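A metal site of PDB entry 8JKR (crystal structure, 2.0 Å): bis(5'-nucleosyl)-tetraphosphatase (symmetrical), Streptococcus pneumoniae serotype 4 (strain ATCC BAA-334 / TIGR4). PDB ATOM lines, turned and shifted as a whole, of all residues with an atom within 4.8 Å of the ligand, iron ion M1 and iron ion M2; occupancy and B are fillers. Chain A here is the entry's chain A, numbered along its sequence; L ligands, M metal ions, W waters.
The side-chain hydroxyl (OG1) of Thr 183 sits at hydrogen-bond distance from an oxygen (O2) of the ligand, 2.5 Å away.
OG1 of Thr 118 lies close to O7 of the ligand (2.6 Å).
An oxygen (O5) of the ligand sits close to the side-chain amide nitrogen (ND2) of Asn 88 (2.9 Å).
The backbone NH (N) of Tyr 180 sits at hydrogen-bond distance from an oxygen (O2) of the ligand (3.4 Å).
Water W6 bridges an oxygen (O8) of the ligand (2.9 Å) and the side-chain amino group of Lys 62 (3.1 Å).
Water W2 bridges the side-chain carboxylate (OD2) of Asp 135 (2.8 Å) and an oxygen (O8) of the ligand (3.2 Å).
Water W5 lies within hydrogen-bond range of an oxygen (O8) of the ligand and the guanidinium group (NH2) of Arg 26.
Water W3 bridges O9 of the ligand (2.8 Å) and O of Thr 118 (3.0 Å).
Water W1 lies within hydrogen-bond range of OD2 of Asp 135 (3.2 Å) and O9 of the ligand (3.2 Å).
Iron ion M2 is bound by water W2 (1.9 Å), a ring nitrogen (NE2) of His 29 (2.0 Å), water W5 (2.1 Å), the side-chain carboxylate (OD1) of Asp 135 (2.2 Å), a ring nitrogen (NE2) of His 58 (2.2 Å) and the side-chain carboxylate (OD2) of Asp 59 (2.3 Å).
Iron ion M2 has six donor atoms within binding distance.
Merely in contact with iron ion M1: Thr 118.
Within 4 Å of iron ion M1: Asp 59, His 91, His 117 and Thr 118.
Along chain A the residues within 4 Å of iron ion M1 span positions 59 to 118.
The nearest printed residue that does not touch iron ion M1 is His 58 (4.03 Å).
A ring nitrogen (NE2) of His 117 sits close to the side-chain hydroxyl (OG1) of Thr 118.
OD2 of Asp 59 lies close to NH2 of Arg 26 (3.1 Å).
The backbone carbonyl oxygen of Asn 88 lies within hydrogen-bond range of a ring nitrogen (ND1) of His 91 (3.1 Å).
OG1 of Thr 183 sits close to O of Tyr 180 (3.5 Å).
OG1 of Thr 168 sits at hydrogen-bond distance from O of Glu 164, at 3.1 Å.
Merely in contact with the ligand: Leu 172, Thr 168 and Val 119.
Within 4 Å of the ligand: Asn 88, His 91, His 117, Thr 118, Val 119, Asp 135, Thr 168, Leu 172, Tyr 180 and Thr 183.
The nearest printed residue that does not touch the ligand is Lys 62 (4.1 Å).
Iron ion M1 is bound by water W6 (2.0 Å), water W2 (2.0 Å), NE2 of His 117 (2.2 Å), OD1 of Asp 59 (2.2 Å), NE2 of His 91 (2.2 Å) and O7 of the ligand (2.2 Å).
The nearest printed residue that does not touch iron ion M2 is Arg 26 (4.03 Å).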
ATOM      1  N   ARG A  26     -16.816  -3.979  -3.233  1.00  0.00           N
ATOM      2  CA  ARG A  26     -17.900  -4.897  -3.587  1.00  0.00           C
ATOM      3  C   ARG A  26     -17.658  -5.593  -4.946  1.00  0.00           C
ATOM      4  O   ARG A  26     -17.937  -6.800  -5.103  1.00  0.00           O
ATOM      5  CB  ARG A  26     -19.262  -4.166  -3.539  1.00  0.00           C
ATOM      6  CG  ARG A  26     -20.512  -5.049  -3.677  1.00  0.00           C
ATOM      7  CD  ARG A  26     -20.521  -6.242  -2.720  1.00  0.00           C
ATOM      8  NE  ARG A  26     -20.538  -5.803  -1.320  1.00  0.00           N
ATOM      9  CZ  ARG A  26     -20.538  -6.597  -0.253  1.00  0.00           C
ATOM     10  NH1 ARG A  26     -20.565  -6.046   0.941  1.00  0.00           N
ATOM     11  NH2 ARG A  26     -20.538  -7.921  -0.374  1.00  0.00           N
ATOM     12  N   HIS A  29     -14.807  -8.063  -4.430  1.00  0.00           N
ATOM     13  CA  HIS A  29     -15.478  -9.221  -3.801  1.00  0.00           C
ATOM     14  C   HIS A  29     -16.096 -10.126  -4.867  1.00  0.00           C
ATOM     15  O   HIS A  29     -15.835 -11.321  -4.888  1.00  0.00           O
ATOM     16  CB  HIS A  29     -16.529  -8.770  -2.772  1.00  0.00           C
ATOM     17  CG  HIS A  29     -17.489  -9.848  -2.341  1.00  0.00           C
ATOM     18  ND1 HIS A  29     -17.081 -10.940  -1.604  1.00  0.00           N
ATOM     19  CD2 HIS A  29     -18.821  -9.991  -2.531  1.00  0.00           C
ATOM     20  CE1 HIS A  29     -18.126 -11.708  -1.345  1.00  0.00           C
ATOM     21  NE2 HIS A  29     -19.194 -11.164  -1.898  1.00  0.00           N
ATOM     22  N   VAL A  33     -15.346 -13.976  -5.836  1.00  0.00           N
ATOM     23  CA  VAL A  33     -16.361 -15.042  -5.834  1.00  0.00           C
ATOM     24  C   VAL A  33     -16.385 -15.750  -7.180  1.00  0.00           C
ATOM     25  O   VAL A  33     -16.542 -16.969  -7.223  1.00  0.00           O
ATOM     26  CB  VAL A  33     -17.776 -14.529  -5.423  1.00  0.00           C
ATOM     27  CG1 VAL A  33     -18.834 -15.633  -5.465  1.00  0.00           C
ATOM     28  CG2 VAL A  33     -17.746 -13.952  -3.993  1.00  0.00           C
ATOM     29  N   HIS A  58     -23.472 -12.540  -8.217  1.00  0.00           N
ATOM     30  CA  HIS A  58     -24.318 -12.814  -7.054  1.00  0.00           C
ATOM     31  C   HIS A  58     -24.696 -11.549  -6.237  1.00  0.00           C
ATOM     32  O   HIS A  58     -25.812 -11.465  -5.721  1.00  0.00           O
ATOM     33  CB  HIS A  58     -23.690 -13.871  -6.160  1.00  0.00           C
ATOM     34  CG  HIS A  58     -22.639 -13.304  -5.263  1.00  0.00           C
ATOM     35  ND1 HIS A  58     -21.431 -12.864  -5.740  1.00  0.00           N
ATOM     36  CD2 HIS A  58     -22.650 -13.035  -3.939  1.00  0.00           C
ATOM     37  CE1 HIS A  58     -20.726 -12.369  -4.746  1.00  0.00           C
ATOM     38  NE2 HIS A  58     -21.440 -12.477  -3.645  1.00  0.00           N
ATOM     39  N   ASP A  59     -23.764 -10.583  -6.137  1.00  0.00           N
ATOM     40  CA  ASP A  59     -24.001  -9.327  -5.420  1.00  0.00           C
ATOM     41  C   ASP A  59     -24.248  -8.116  -6.323  1.00  0.00           C
ATOM     42  O   ASP A  59     -24.064  -6.982  -5.903  1.00  0.00           O
ATOM     43  CB  ASP A  59     -22.879  -9.017  -4.433  1.00  0.00           C
ATOM     44  CG  ASP A  59     -23.071  -9.706  -3.092  1.00  0.00           C
ATOM     45  OD1 ASP A  59     -24.167 -10.232  -2.825  1.00  0.00           O
ATOM     46  OD2 ASP A  59     -22.096  -9.756  -2.327  1.00  0.00           O
ATOM     47  N   LYS A  62     -26.651  -5.510  -4.994  1.00  0.00           N
ATOM     48  CA  LYS A  62     -26.310  -5.197  -3.603  1.00  0.00           C
ATOM     49  C   LYS A  62     -26.732  -3.795  -3.180  1.00  0.00           C
ATOM     50  O   LYS A  62     -27.213  -3.599  -2.052  1.00  0.00           O
ATOM     51  CB  LYS A  62     -24.805  -5.400  -3.366  1.00  0.00           C
ATOM     52  CG  LYS A  62     -24.312  -5.252  -1.928  1.00  0.00           C
ATOM     53  CD  LYS A  62     -24.854  -6.312  -0.968  1.00  0.00           C
ATOM     54  CE  LYS A  62     -24.065  -6.304   0.324  1.00  0.00           C
ATOM     55  NZ  LYS A  62     -24.638  -7.242   1.327  1.00  0.00           N
ATOM     56  N   ASN A  88     -30.376  -7.375   3.053  1.00  0.00           N
ATOM     57  CA  ASN A  88     -29.765  -8.693   3.246  1.00  0.00           C
ATOM     58  C   ASN A  88     -30.515  -9.817   2.567  1.00  0.00           C
ATOM     59  O   ASN A  88     -29.912 -10.623   1.840  1.00  0.00           O
ATOM     60  CB  ASN A  88     -29.596  -9.000   4.744  1.00  0.00           C
ATOM     61  CG  ASN A  88     -28.523  -8.137   5.378  1.00  0.00           C
ATOM     62  OD1 ASN A  88     -27.844  -7.397   4.694  1.00  0.00           O
ATOM     63  ND2 ASN A  88     -28.340  -8.272   6.674  1.00  0.00           N
ATOM     64  N   HIS A  91     -31.425  -8.564  -1.819  1.00  0.00           N
ATOM     65  CA  HIS A  91     -30.423  -8.408  -2.899  1.00  0.00           C
ATOM     66  C   HIS A  91     -30.244  -9.664  -3.754  1.00  0.00           C
ATOM     67  O   HIS A  91     -30.045  -9.572  -4.972  1.00  0.00           O
ATOM     68  CB  HIS A  91     -29.106  -7.766  -2.399  1.00  0.00           C
ATOM     69  CG  HIS A  91     -28.180  -8.695  -1.667  1.00  0.00           C
ATOM     70  ND1 HIS A  91     -28.338  -9.011  -0.331  1.00  0.00           N
ATOM     71  CD2 HIS A  91     -27.050  -9.312  -2.076  1.00  0.00           C
ATOM     72  CE1 HIS A  91     -27.347  -9.803   0.044  1.00  0.00           C
ATOM     73  NE2 HIS A  91     -26.561 -10.007  -0.994  1.00  0.00           N
ATOM     74  N   HIS A 117     -28.297 -17.145  -2.401  1.00  0.00           N
ATOM     75  CA  HIS A 117     -26.894 -17.106  -1.990  1.00  0.00           C
ATOM     76  C   HIS A 117     -26.681 -16.632  -0.547  1.00  0.00           C
ATOM     77  O   HIS A 117     -25.680 -16.969   0.061  1.00  0.00           O
ATOM     78  CB  HIS A 117     -26.013 -16.300  -2.958  1.00  0.00           C
ATOM     79  CG  HIS A 117     -26.075 -14.819  -2.753  1.00  0.00           C
ATOM     80  ND1 HIS A 117     -26.976 -14.017  -3.441  1.00  0.00           N
ATOM     81  CD2 HIS A 117     -25.348 -13.987  -1.978  1.00  0.00           C
ATOM     82  CE1 HIS A 117     -26.793 -12.757  -3.082  1.00  0.00           C
ATOM     83  NE2 HIS A 117     -25.816 -12.708  -2.201  1.00  0.00           N
ATOM     84  N   THR A 118     -27.618 -15.852  -0.024  1.00  0.00           N
ATOM     85  CA  THR A 118     -27.523 -15.312   1.349  1.00  0.00           C
ATOM     86  C   THR A 118     -28.135 -16.258   2.383  1.00  0.00           C
ATOM     87  O   THR A 118     -27.545 -16.491   3.435  1.00  0.00           O
ATOM     88  CB  THR A 118     -28.215 -13.936   1.446  1.00  0.00           C
ATOM     89  OG1 THR A 118     -27.677 -13.054   0.454  1.00  0.00           O
ATOM     90  CG2 THR A 118     -28.074 -13.326   2.824  1.00  0.00           C
ATOM     91  N   VAL A 119     -29.291 -16.834   2.056  1.00  0.00           N
ATOM     92  CA  VAL A 119     -30.127 -17.569   3.041  1.00  0.00           C
ATOM     93  C   VAL A 119     -30.146 -19.088   2.830  1.00  0.00           C
ATOM     94  O   VAL A 119     -30.574 -19.846   3.720  1.00  0.00           O
ATOM     95  CB  VAL A 119     -31.562 -16.972   3.090  1.00  0.00           C
ATOM     96  CG1 VAL A 119     -31.507 -15.480   3.412  1.00  0.00           C
ATOM     97  CG2 VAL A 119     -32.308 -17.220   1.774  1.00  0.00           C
ATOM     98  N   ASP A 135     -18.860 -17.436  -1.961  1.00  0.00           N
ATOM     99  CA  ASP A 135     -19.149 -16.118  -1.399  1.00  0.00           C
ATOM    100  C   ASP A 135     -18.381 -15.912  -0.080  1.00  0.00           C
ATOM    101  O   ASP A 135     -17.780 -14.854   0.182  1.00  0.00           O
ATOM    102  CB  ASP A 135     -20.668 -15.997  -1.193  1.00  0.00           C
ATOM    103  CG  ASP A 135     -21.101 -14.618  -0.740  1.00  0.00           C
ATOM    104  OD1 ASP A 135     -20.398 -13.636  -1.022  1.00  0.00           O
ATOM    105  OD2 ASP A 135     -22.168 -14.532  -0.087  1.00  0.00           O
ATOM    106  N   GLU A 164     -20.779 -22.654   7.295  1.00  0.00           N
ATOM    107  CA  GLU A 164     -21.146 -21.261   6.998  1.00  0.00           C
ATOM    108  C   GLU A 164     -22.497 -20.923   7.638  1.00  0.00           C
ATOM    109  O   GLU A 164     -22.599 -19.908   8.337  1.00  0.00           O
ATOM    110  CB  GLU A 164     -21.212 -21.001   5.500  1.00  0.00           C
ATOM    111  CG  GLU A 164     -21.676 -19.577   5.206  1.00  0.00           C
ATOM    112  CD  GLU A 164     -21.712 -19.212   3.733  1.00  0.00           C
ATOM    113  OE1 GLU A 164     -21.211 -19.986   2.864  1.00  0.00           O
ATOM    114  OE2 GLU A 164     -22.251 -18.114   3.439  1.00  0.00           O
ATOM    115  N   THR A 168     -23.322 -18.147  10.598  1.00  0.00           N
ATOM    116  CA  THR A 168     -24.217 -17.002  10.316  1.00  0.00           C
ATOM    117  C   THR A 168     -25.350 -16.904  11.348  1.00  0.00           C
ATOM    118  O   THR A 168     -25.557 -15.837  11.944  1.00  0.00           O
ATOM    119  CB  THR A 168     -24.773 -17.105   8.877  1.00  0.00           C
ATOM    120  OG1 THR A 168     -23.675 -16.983   7.975  1.00  0.00           O
ATOM    121  CG2 THR A 168     -25.802 -15.991   8.551  1.00  0.00           C
ATOM    122  N   TYR A 171     -23.822 -15.879  14.632  1.00  0.00           N
ATOM    123  CA  TYR A 171     -23.460 -14.456  14.605  1.00  0.00           C
ATOM    124  C   TYR A 171     -24.695 -13.527  14.664  1.00  0.00           C
ATOM    125  O   TYR A 171     -24.680 -12.550  15.415  1.00  0.00           O
ATOM    126  CB  TYR A 171     -22.558 -14.140  13.415  1.00  0.00           C
ATOM    127  CG  TYR A 171     -22.321 -12.656  13.179  1.00  0.00           C
ATOM    128  CD1 TYR A 171     -21.341 -11.952  13.895  1.00  0.00           C
ATOM    129  CD2 TYR A 171     -23.071 -11.965  12.212  1.00  0.00           C
ATOM    130  CE1 TYR A 171     -21.114 -10.597  13.662  1.00  0.00           C
ATOM    131  CE2 TYR A 171     -22.856 -10.614  11.985  1.00  0.00           C
ATOM    132  CZ  TYR A 171     -21.883  -9.937  12.703  1.00  0.00           C
ATOM    133  OH  TYR A 171     -21.695  -8.590  12.451  1.00  0.00           O
ATOM    134  N   LEU A 172     -25.746 -13.845  13.905  1.00  0.00           N
ATOM    135  CA  LEU A 172     -26.967 -13.036  13.905  1.00  0.00           C
ATOM    136  C   LEU A 172     -27.644 -13.052  15.272  1.00  0.00           C
ATOM    137  O   LEU A 172     -28.085 -11.986  15.719  1.00  0.00           O
ATOM    138  CB  LEU A 172     -27.927 -13.466  12.792  1.00  0.00           C
ATOM    139  CG  LEU A 172     -27.437 -13.182  11.365  1.00  0.00           C
ATOM    140  CD1 LEU A 172     -28.424 -13.776  10.366  1.00  0.00           C
ATOM    141  CD2 LEU A 172     -27.227 -11.686  11.117  1.00  0.00           C
ATOM    142  N   PRO A 178     -32.638  -9.993  13.295  1.00  0.00           N
ATOM    143  CA  PRO A 178     -33.632 -10.985  12.864  1.00  0.00           C
ATOM    144  C   PRO A 178     -32.968 -12.004  11.932  1.00  0.00           C
ATOM    145  O   PRO A 178     -31.964 -11.686  11.276  1.00  0.00           O
ATOM    146  CB  PRO A 178     -34.693 -10.173  12.100  1.00  0.00           C
ATOM    147  CG  PRO A 178     -34.484  -8.753  12.512  1.00  0.00           C
ATOM    148  CD  PRO A 178     -33.018  -8.617  12.876  1.00  0.00           C
ATOM    149  N   ILE A 179     -33.503 -13.213  11.917  1.00  0.00           N
ATOM    150  CA  ILE A 179     -33.004 -14.291  11.077  1.00  0.00           C
ATOM    151  C   ILE A 179     -34.116 -14.744  10.140  1.00  0.00           C
ATOM    152  O   ILE A 179     -35.178 -15.210  10.584  1.00  0.00           O
ATOM    153  CB  ILE A 179     -32.506 -15.480  11.942  1.00  0.00           C
ATOM    154  CG1 ILE A 179     -31.273 -15.075  12.781  1.00  0.00           C
ATOM    155  CG2 ILE A 179     -32.189 -16.700  11.059  1.00  0.00           C
ATOM    156  CD1 ILE A 179     -30.988 -15.994  13.958  1.00  0.00           C
ATOM    157  N   TYR A 180     -33.866 -14.638   8.834  1.00  0.00           N
ATOM    158  CA  TYR A 180     -34.842 -15.044   7.838  1.00  0.00           C
ATOM    159  C   TYR A 180     -35.162 -16.527   8.017  1.00  0.00           C
ATOM    160  O   TYR A 180     -34.244 -17.337   8.132  1.00  0.00           O
ATOM    161  CB  TYR A 180     -34.333 -14.757   6.421  1.00  0.00           C
ATOM    162  CG  TYR A 180     -35.421 -14.781   5.376  1.00  0.00           C
ATOM    163  CD1 TYR A 180     -36.474 -13.857   5.405  1.00  0.00           C
ATOM    164  CD2 TYR A 180     -35.418 -15.747   4.367  1.00  0.00           C
ATOM    165  CE1 TYR A 180     -37.476 -13.886   4.453  1.00  0.00           C
ATOM    166  CE2 TYR A 180     -36.435 -15.792   3.421  1.00  0.00           C
ATOM    167  CZ  TYR A 180     -37.456 -14.853   3.461  1.00  0.00           C
ATOM    168  OH  TYR A 180     -38.451 -14.898   2.512  1.00  0.00           O
ATOM    169  N   THR A 183     -33.320 -19.262   6.169  1.00  0.00           N
ATOM    170  CA  THR A 183     -31.962 -19.514   6.695  1.00  0.00           C
ATOM    171  C   THR A 183     -31.958 -20.670   7.684  1.00  0.00           C
ATOM    172  O   THR A 183     -31.031 -21.503   7.666  1.00  0.00           O
ATOM    173  CB  THR A 183     -31.338 -18.256   7.314  1.00  0.00           C
ATOM    174  OG1 THR A 183     -31.299 -17.236   6.315  1.00  0.00           O
ATOM    175  CG2 THR A 183     -29.911 -18.498   7.819  1.00  0.00           C
HETATM  176  N1  LIG L   1     -27.960 -12.252   6.845  1.00  0.00           N
HETATM  177  C1  LIG L   1     -29.227 -11.910   7.374  1.00  0.00           C
HETATM  178  N2  LIG L   1     -30.189 -12.830   7.494  1.00  0.00           N
HETATM  179  C2  LIG L   1     -29.956 -14.089   7.088  1.00  0.00           C
HETATM  180  C3  LIG L   1     -28.696 -14.458   6.561  1.00  0.00           C
HETATM  181  C4  LIG L   1     -27.692 -13.498   6.435  1.00  0.00           C
HETATM  182  O1  LIG L   1     -29.442 -10.733   7.751  1.00  0.00           O
HETATM  183  O2  LIG L   1     -30.902 -14.888   7.214  1.00  0.00           O
HETATM  184  C5  LIG L   1     -26.913 -11.246   6.769  1.00  0.00           C
HETATM  185  C6  LIG L   1     -25.522 -11.859   6.940  1.00  0.00           C
HETATM  186  O3  LIG L   1     -24.993 -11.539   8.221  1.00  0.00           O
HETATM  187  C7  LIG L   1     -24.719 -11.241   5.815  1.00  0.00           C
HETATM  188  C8  LIG L   1     -25.668 -10.380   5.010  1.00  0.00           C
HETATM  189  O4  LIG L   1     -23.694 -10.355   6.280  1.00  0.00           O
HETATM  190  O5  LIG L   1     -26.991 -10.568   5.520  1.00  0.00           O
HETATM  191  C9  LIG L   1     -25.601 -10.638   3.504  1.00  0.00           C
HETATM  192  O6  LIG L   1     -25.220 -11.990   3.314  1.00  0.00           O
HETATM  193  P1  LIG L   1     -24.348 -12.478   2.076  1.00  0.00           P
HETATM  194  O7  LIG L   1     -25.321 -12.203   0.947  1.00  0.00           O
HETATM  195  O8  LIG L   1     -23.117 -11.634   2.216  1.00  0.00           O
HETATM  196  O9  LIG L   1     -24.083 -13.931   2.396  1.00  0.00           O
HETATM  197 FE    FE M   1     -24.761 -11.253  -1.005  1.00  0.00          FE
HETATM  198 FE    FE M   2     -21.135 -11.702  -1.639  1.00  0.00          FE
HETATM  199  O   HOH W   1     -20.937 -14.323   2.823  1.00  0.00           O
HETATM  200  O   HOH W   2     -22.886 -12.012  -0.929  1.00  0.00           O
HETATM  201  O   HOH W   3     -25.281 -14.968   4.656  1.00  0.00           O
HETATM  202  O   HOH W   4     -23.514 -16.421   1.392  1.00  0.00           O
HETATM  203  O   HOH W   5     -20.798 -11.138   0.387  1.00  0.00           O
HETATM  204  O   HOH W   6     -23.656  -9.858  -0.045  1.00  0.00           O
